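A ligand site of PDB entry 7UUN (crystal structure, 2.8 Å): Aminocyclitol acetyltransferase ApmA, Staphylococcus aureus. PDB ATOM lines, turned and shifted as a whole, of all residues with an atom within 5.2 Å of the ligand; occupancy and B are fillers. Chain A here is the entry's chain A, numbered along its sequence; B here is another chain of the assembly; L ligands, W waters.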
ATOM      1  N   ASP A 107       9.666  15.077   4.898  1.00  0.00           N
ATOM      2  CA  ASP A 107       9.766  16.496   5.220  1.00  0.00           C
ATOM      3  C   ASP A 107       9.704  16.756   6.715  1.00  0.00           C
ATOM      4  O   ASP A 107      10.278  17.743   7.189  1.00  0.00           O
ATOM      5  CB  ASP A 107       8.651  17.268   4.505  1.00  0.00           C
ATOM      6  CG  ASP A 107       9.005  17.622   3.082  1.00  0.00           C
ATOM      7  OD1 ASP A 107      10.158  18.052   2.845  1.00  0.00           O
ATOM      8  OD2 ASP A 107       8.142  17.464   2.204  1.00  0.00           O
ATOM      9  N   GLY A 111      12.748  18.704   8.589  1.00  0.00           N
ATOM     10  CA  GLY A 111      12.249  19.789   9.420  1.00  0.00           C
ATOM     11  C   GLY A 111      12.796  19.727  10.826  1.00  0.00           C
ATOM     12  O   GLY A 111      13.246  20.728  11.385  1.00  0.00           O
ATOM     13  N   GLU A 114      16.530  20.772  10.780  1.00  0.00           N
ATOM     14  CA  GLU A 114      16.744  22.216  10.804  1.00  0.00           C
ATOM     15  C   GLU A 114      16.593  22.774  12.217  1.00  0.00           C
ATOM     16  O   GLU A 114      17.392  23.624  12.648  1.00  0.00           O
ATOM     17  CB  GLU A 114      15.773  22.899   9.839  1.00  0.00           C
ATOM     18  CG  GLU A 114      16.030  24.373   9.605  1.00  0.00           C
ATOM     19  CD  GLU A 114      15.089  24.972   8.568  1.00  0.00           C
ATOM     20  OE1 GLU A 114      14.094  24.301   8.207  1.00  0.00           O
ATOM     21  OE2 GLU A 114      15.347  26.101   8.111  1.00  0.00           O
ATOM     22  N   ASN A 115      15.584  22.298  12.961  1.00  0.00           N
ATOM     23  CA  ASN A 115      15.422  22.717  14.345  1.00  0.00           C
ATOM     24  C   ASN A 115      16.567  22.244  15.234  1.00  0.00           C
ATOM     25  O   ASN A 115      16.732  22.756  16.341  1.00  0.00           O
ATOM     26  CB  ASN A 115      14.104  22.167  14.919  1.00  0.00           C
ATOM     27  CG  ASN A 115      12.886  22.621  14.119  1.00  0.00           C
ATOM     28  OD1 ASN A 115      12.787  23.785  13.713  1.00  0.00           O
ATOM     29  ND2 ASN A 115      11.950  21.706  13.903  1.00  0.00           N
ATOM     30  N   TYR A 117      16.821  19.060  16.363  1.00  0.00           N
ATOM     31  CA  TYR A 117      16.346  18.023  17.268  1.00  0.00           C
ATOM     32  C   TYR A 117      17.121  16.719  17.145  1.00  0.00           C
ATOM     33  O   TYR A 117      16.920  15.825  17.970  1.00  0.00           O
ATOM     34  CB  TYR A 117      14.863  17.725  17.007  1.00  0.00           C
ATOM     35  CG  TYR A 117      13.927  18.867  17.337  1.00  0.00           C
ATOM     36  CD1 TYR A 117      14.365  19.973  18.050  1.00  0.00           C
ATOM     37  CD2 TYR A 117      12.602  18.830  16.936  1.00  0.00           C
ATOM     38  CE1 TYR A 117      13.513  21.002  18.350  1.00  0.00           C
ATOM     39  CE2 TYR A 117      11.742  19.852  17.228  1.00  0.00           C
ATOM     40  CZ  TYR A 117      12.199  20.943  17.935  1.00  0.00           C
ATOM     41  OH  TYR A 117      11.333  21.977  18.233  1.00  0.00           O
ATOM     42  N   GLU A 132       6.805  12.131  11.716  1.00  0.00           N
ATOM     43  CA  GLU A 132       6.992  13.468  12.259  1.00  0.00           C
ATOM     44  C   GLU A 132       7.767  13.387  13.563  1.00  0.00           C
ATOM     45  O   GLU A 132       7.652  12.426  14.317  1.00  0.00           O
ATOM     46  CB  GLU A 132       5.653  14.182  12.498  1.00  0.00           C
ATOM     47  CG  GLU A 132       4.932  14.589  11.215  1.00  0.00           C
ATOM     48  CD  GLU A 132       5.401  15.930  10.680  1.00  0.00           C
ATOM     49  OE1 GLU A 132       6.247  16.575  11.329  1.00  0.00           O
ATOM     50  OE2 GLU A 132       4.910  16.355   9.613  1.00  0.00           O
ATOM     51  N   HIS A 134       8.479  16.064  16.695  1.00  0.00           N
ATOM     52  CA  HIS A 134       8.227  17.353  17.303  1.00  0.00           C
ATOM     53  C   HIS A 134       8.633  17.311  18.770  1.00  0.00           C
ATOM     54  O   HIS A 134       8.604  16.264  19.409  1.00  0.00           O
ATOM     55  CB  HIS A 134       6.753  17.745  17.196  1.00  0.00           C
ATOM     56  CG  HIS A 134       6.340  18.133  15.815  1.00  0.00           C
ATOM     57  ND1 HIS A 134       7.197  18.084  14.735  1.00  0.00           N
ATOM     58  CD2 HIS A 134       5.159  18.584  15.334  1.00  0.00           C
ATOM     59  CE1 HIS A 134       6.553  18.477  13.647  1.00  0.00           C
ATOM     60  NE2 HIS A 134       5.324  18.782  13.987  1.00  0.00           N
ATOM     61  N   ALA A 135       9.043  18.471  19.275  1.00  0.00           N
ATOM     62  CA  ALA A 135       9.280  18.609  20.702  1.00  0.00           C
ATOM     63  C   ALA A 135       7.966  18.886  21.408  1.00  0.00           C
ATOM     64  O   ALA A 135       6.889  18.948  20.793  1.00  0.00           O
ATOM     65  CB  ALA A 135      10.307  19.716  20.953  1.00  0.00           C
ATOM     66  N   HIS A 137       5.764  21.442  24.146  1.00  0.00           N
ATOM     67  CA  HIS A 137       5.725  22.785  24.682  1.00  0.00           C
ATOM     68  C   HIS A 137       5.987  22.736  26.182  1.00  0.00           C
ATOM     69  O   HIS A 137       6.115  21.662  26.796  1.00  0.00           O
ATOM     70  CB  HIS A 137       4.392  23.449  24.349  1.00  0.00           C
ATOM     71  CG  HIS A 137       4.290  23.887  22.924  1.00  0.00           C
ATOM     72  ND1 HIS A 137       3.311  24.759  22.480  1.00  0.00           N
ATOM     73  CD2 HIS A 137       5.045  23.584  21.840  1.00  0.00           C
ATOM     74  CE1 HIS A 137       3.472  24.964  21.190  1.00  0.00           C
ATOM     75  NE2 HIS A 137       4.516  24.257  20.779  1.00  0.00           N
ATOM     76  N   ASP A 146       3.287  28.703  22.129  1.00  0.00           N
ATOM     77  CA  ASP A 146       4.671  29.134  21.935  1.00  0.00           C
ATOM     78  C   ASP A 146       4.748  30.517  21.325  1.00  0.00           C
ATOM     79  O   ASP A 146       5.533  31.349  21.775  1.00  0.00           O
ATOM     80  CB  ASP A 146       5.434  28.118  21.076  1.00  0.00           C
ATOM     81  CG  ASP A 146       4.795  27.880  19.723  1.00  0.00           C
ATOM     82  OD1 ASP A 146       3.600  28.216  19.555  1.00  0.00           O
ATOM     83  OD2 ASP A 146       5.480  27.363  18.827  1.00  0.00           O
ATOM     84  N   ASP A 147       3.899  30.810  20.328  1.00  0.00           N
ATOM     85  CA  ASP A 147       3.980  32.077  19.606  1.00  0.00           C
ATOM     86  C   ASP A 147       3.514  33.280  20.419  1.00  0.00           C
ATOM     87  O   ASP A 147       3.606  34.403  19.920  1.00  0.00           O
ATOM     88  CB  ASP A 147       3.181  32.009  18.306  1.00  0.00           C
ATOM     89  CG  ASP A 147       3.953  31.365  17.180  1.00  0.00           C
ATOM     90  OD1 ASP A 147       5.057  31.855  16.869  1.00  0.00           O
ATOM     91  OD2 ASP A 147       3.471  30.373  16.610  1.00  0.00           O
ATOM     92  N   TYR A 172      10.898  22.041  24.081  1.00  0.00           N
ATOM     93  CA  TYR A 172      11.517  22.600  22.872  1.00  0.00           C
ATOM     94  C   TYR A 172      12.873  21.959  22.588  1.00  0.00           C
ATOM     95  O   TYR A 172      13.695  22.552  21.877  1.00  0.00           O
ATOM     96  CB  TYR A 172      11.640  24.124  22.973  1.00  0.00           C
ATOM     97  CG  TYR A 172      10.328  24.852  23.195  1.00  0.00           C
ATOM     98  CD1 TYR A 172       9.118  24.230  22.895  1.00  0.00           C
ATOM     99  CD2 TYR A 172      10.294  26.145  23.701  1.00  0.00           C
ATOM    100  CE1 TYR A 172       7.920  24.879  23.098  1.00  0.00           C
ATOM    101  CE2 TYR A 172       9.098  26.804  23.906  1.00  0.00           C
ATOM    102  CZ  TYR A 172       7.913  26.165  23.608  1.00  0.00           C
ATOM    103  OH  TYR A 172       6.706  26.806  23.803  1.00  0.00           O
ATOM    104  N   ASP B  57       6.069  28.814   1.351  1.00  0.00           N
ATOM    105  CA  ASP B  57       6.934  28.855   2.529  1.00  0.00           C
ATOM    106  C   ASP B  57       8.385  28.590   2.147  1.00  0.00           C
ATOM    107  O   ASP B  57       9.302  29.114   2.799  1.00  0.00           O
ATOM    108  CB  ASP B  57       6.475  27.854   3.574  1.00  0.00           C
ATOM    109  CG  ASP B  57       6.772  28.329   4.995  1.00  0.00           C
ATOM    110  OD1 ASP B  57       6.108  29.300   5.444  1.00  0.00           O
ATOM    111  OD2 ASP B  57       7.683  27.759   5.637  1.00  0.00           O
ATOM    112  N   GLU B  87       0.017  32.284  11.837  1.00  0.00           N
ATOM    113  CA  GLU B  87      -0.187  33.188  12.960  1.00  0.00           C
ATOM    114  C   GLU B  87      -0.161  34.635  12.496  1.00  0.00           C
ATOM    115  O   GLU B  87       0.420  34.983  11.465  1.00  0.00           O
ATOM    116  CB  GLU B  87       0.871  32.971  14.036  1.00  0.00           C
ATOM    117  CG  GLU B  87       2.223  33.594  13.726  1.00  0.00           C
ATOM    118  CD  GLU B  87       3.217  32.601  13.160  1.00  0.00           C
ATOM    119  OE1 GLU B  87       2.774  31.528  12.705  1.00  0.00           O
ATOM    120  OE2 GLU B  87       4.433  32.893  13.160  1.00  0.00           O
ATOM    121  N   TYR B 104      -2.070  29.562  14.881  1.00  0.00           N
ATOM    122  CA  TYR B 104      -1.780  28.948  13.604  1.00  0.00           C
ATOM    123  C   TYR B 104      -2.419  27.573  13.538  1.00  0.00           C
ATOM    124  O   TYR B 104      -2.785  26.966  14.541  1.00  0.00           O
ATOM    125  CB  TYR B 104      -0.265  28.821  13.364  1.00  0.00           C
ATOM    126  CG  TYR B 104       0.484  28.110  14.479  1.00  0.00           C
ATOM    127  CD1 TYR B 104       0.979  28.831  15.558  1.00  0.00           C
ATOM    128  CD2 TYR B 104       0.672  26.740  14.451  1.00  0.00           C
ATOM    129  CE1 TYR B 104       1.654  28.197  16.582  1.00  0.00           C
ATOM    130  CE2 TYR B 104       1.361  26.093  15.462  1.00  0.00           C
ATOM    131  CZ  TYR B 104       1.846  26.828  16.527  1.00  0.00           C
ATOM    132  OH  TYR B 104       2.525  26.204  17.551  1.00  0.00           O
ATOM    133  N   ASN B 128      -1.157  21.789  15.147  1.00  0.00           N
ATOM    134  CA  ASN B 128      -0.164  21.215  14.258  1.00  0.00           C
ATOM    135  C   ASN B 128      -0.675  21.156  12.830  1.00  0.00           C
ATOM    136  O   ASN B 128      -1.868  20.982  12.574  1.00  0.00           O
ATOM    137  CB  ASN B 128       0.202  19.804  14.714  1.00  0.00           C
ATOM    138  CG  ASN B 128       1.450  19.291  14.060  1.00  0.00           C
ATOM    139  OD1 ASN B 128       1.446  18.897  12.900  1.00  0.00           O
ATOM    140  ND2 ASN B 128       2.542  19.340  14.796  1.00  0.00           N
ATOM    141  N   GLY B 129       0.261  21.294  11.882  1.00  0.00           N
ATOM    142  CA  GLY B 129      -0.126  21.244  10.477  1.00  0.00           C
ATOM    143  C   GLY B 129      -0.806  19.945  10.103  1.00  0.00           C
ATOM    144  O   GLY B 129      -1.731  19.943   9.289  1.00  0.00           O
ATOM    145  N   THR B 130      -0.369  18.836  10.704  1.00  0.00           N
ATOM    146  CA  THR B 130      -0.865  17.525  10.288  1.00  0.00           C
ATOM    147  C   THR B 130      -2.271  17.243  10.771  1.00  0.00           C
ATOM    148  O   THR B 130      -2.915  16.330  10.242  1.00  0.00           O
ATOM    149  CB  THR B 130       0.072  16.431  10.794  1.00  0.00           C
ATOM    150  OG1 THR B 130       0.309  16.613  12.194  1.00  0.00           O
ATOM    151  CG2 THR B 130       1.399  16.464  10.047  1.00  0.00           C
HETATM  152  C1  LIG L   1       5.783  24.605  15.425  1.00  0.00           C
HETATM  153  O1  LIG L   1       5.352  25.930  15.612  1.00  0.00           O
HETATM  154  C2  LIG L   1       5.562  23.778  16.656  1.00  0.00           C
HETATM  155  N1  LIG L   1       4.181  23.807  17.050  1.00  0.00           N
HETATM  156  C3  LIG L   1       6.390  24.285  17.810  1.00  0.00           C
HETATM  157  O2  LIG L   1       6.533  23.234  18.741  1.00  0.00           O
HETATM  158  C4  LIG L   1       7.802  24.569  17.413  1.00  0.00           C
HETATM  159  O3  LIG L   1       8.325  25.358  18.464  1.00  0.00           O
HETATM  160  C5  LIG L   1       7.864  25.357  16.138  1.00  0.00           C
HETATM  161  O4  LIG L   1       7.166  24.638  15.162  1.00  0.00           O
HETATM  162  C6  LIG L   1       9.294  25.465  15.693  1.00  0.00           C
HETATM  163  C7  LIG L   1       4.188  28.375  12.467  1.00  0.00           C
HETATM  164  N2  LIG L   1       4.340  29.360  11.434  1.00  0.00           N
HETATM  165  C8  LIG L   1       4.982  27.149  12.093  1.00  0.00           C
HETATM  166  C9  LIG L   1       5.126  26.155  13.220  1.00  0.00           C
HETATM  167  O5  LIG L   1       6.198  25.323  12.856  1.00  0.00           O
HETATM  168  C10 LIG L   1       5.549  26.805  14.515  1.00  0.00           C
HETATM  169  C11 LIG L   1       4.697  28.001  14.809  1.00  0.00           C
HETATM  170  N3  LIG L   1       5.276  28.666  15.925  1.00  0.00           N
HETATM  171  C12 LIG L   1       4.744  29.006  13.707  1.00  0.00           C
HETATM  172  C13 LIG L   1       6.034  24.588  11.675  1.00  0.00           C
HETATM  173  C14 LIG L   1       6.679  23.230  11.740  1.00  0.00           C
HETATM  174  C15 LIG L   1       6.067  22.622  10.523  1.00  0.00           C
HETATM  175  C16 LIG L   1       4.631  22.971  10.840  1.00  0.00           C
HETATM  176  O6  LIG L   1       4.682  24.244  11.455  1.00  0.00           O
HETATM  177  C17 LIG L   1       4.006  21.977  11.807  1.00  0.00           C
HETATM  178  C18 LIG L   1       9.948  23.929   7.719  1.00  0.00           C
HETATM  179  C19 LIG L   1       9.378  22.550   7.484  1.00  0.00           C
HETATM  180  C20 LIG L   1       7.884  22.567   7.742  1.00  0.00           C
HETATM  181  C21 LIG L   1       7.557  23.613   8.778  1.00  0.00           C
HETATM  182  O7  LIG L   1       6.278  23.375   9.343  1.00  0.00           O
HETATM  183  C22 LIG L   1       9.734  24.345   9.168  1.00  0.00           C
HETATM  184  O8  LIG L   1       8.603  23.688   9.724  1.00  0.00           O
HETATM  185  C23 LIG L   1      10.937  23.986  10.005  1.00  0.00           C
HETATM  186  N4  LIG L   1       9.572  26.868  15.501  1.00  0.00           N
HETATM  187  O9  LIG L   1       8.087  23.294  11.660  1.00  0.00           O
HETATM  188  O10 LIG L   1       9.654  22.184   6.131  1.00  0.00           O
HETATM  189  O11 LIG L   1      11.342  23.870   7.411  1.00  0.00           O
HETATM  190  O12 LIG L   1       4.170  20.650  11.308  1.00  0.00           O
HETATM  191  O13 LIG L   1       4.263  26.522  11.069  1.00  0.00           O
HETATM  192  N5  LIG L   1      11.360  25.169  10.699  1.00  0.00           N
HETATM  193  N6  LIG L   1       7.442  21.285   8.233  1.00  0.00           N
HETATM  194  O   HOH W   1       1.256  27.352   9.781  1.00  0.00           O
HETATM  195  O   HOH W   2       1.941  22.125  17.364  1.00  0.00           O
HETATM  196  O   HOH W   3       6.170  18.927   8.770  1.00  0.00           O
HETATM  197  O   HOH W   4       8.529  27.686  12.001  1.00  0.00           O
HETATM  198  O   HOH W   5       5.199  27.097   7.974  1.00  0.00           O
HETATM  199  O   HOH W   6       6.829  30.543  11.270  1.00  0.00           O
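OD2 of Asp 147 is in salt-bridge range of N3 of the ligand, 2.6 Å away.
N5 of the ligand lies within salt-bridge range of OE1 of Glu 114 (3.8 Å).
A nitrogen (N1) of the ligand is in hydrogen-bond range of the side-chain hydroxyl (OH) of Tyr 104 of chain B (3.0 Å).
N2 of the ligand is in salt-bridge range of OE1 of Glu 87 of chain B, at 3.0 Å.
An oxygen (O2) of the ligand lies within hydrogen-bond range of a ring nitrogen (NE2) of His 137 (3.0 Å).
A nitrogen (N3) of the ligand lies within salt-bridge range of the side-chain carboxylate of Asp 146 (3.2 Å).
A ring nitrogen (NE2) of His 134 sits at hydrogen-bond distance from an oxygen (O12) of the ligand (3.5 Å).
OH of Tyr 104 of chain B is in hydrogen-bond range of OD1 of Asp 146.
ND2 of Asn 128 of chain B sits close to NE2 of His 134, 3.0 Å away.
The side-chain hydroxyl of Thr 130 of chain B is in hydrogen-bond range of the side-chain amide oxygen of Asn 128 of chain B (2.6 Å).
O of Gly 111 lies within hydrogen-bond range of ND2 of Asn 115, 3.0 Å away.
Asn 115 touches the ligand (OD1 to N5, 3.6 Å).
Asn 128 of chain B touches the ligand (OD1 to O12, 3.6 Å).
N of Gly 129 of chain B touches C17 of the ligand, 3.8 Å away.
Hydrophobic or aromatic side chains within 4 Å of the ligand: His 134, His 137 and Tyr 104 of chain B.
Ten residues have an atom within 4 Å of the ligand: Glu 114, Asn 115, His 134, His 137, Asp 146, Asp 147, Glu 87 of chain B, Tyr 104 of chain B, Asn 128 of chain B and Gly 129 of chain B.
Along chain A the residues within 4 Å of the ligand span positions 114 to 147.
The nearest printed residue that does not touch the ligand is Gly 111 (4.2 Å).
Water W3 lies within hydrogen-bond range of a nitrogen (N6) of the ligand and the side-chain carboxylate of Glu 132.
Water W5 lies within hydrogen-bond range of O13 of the ligand and OD2 of Asp 57 of chain B.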
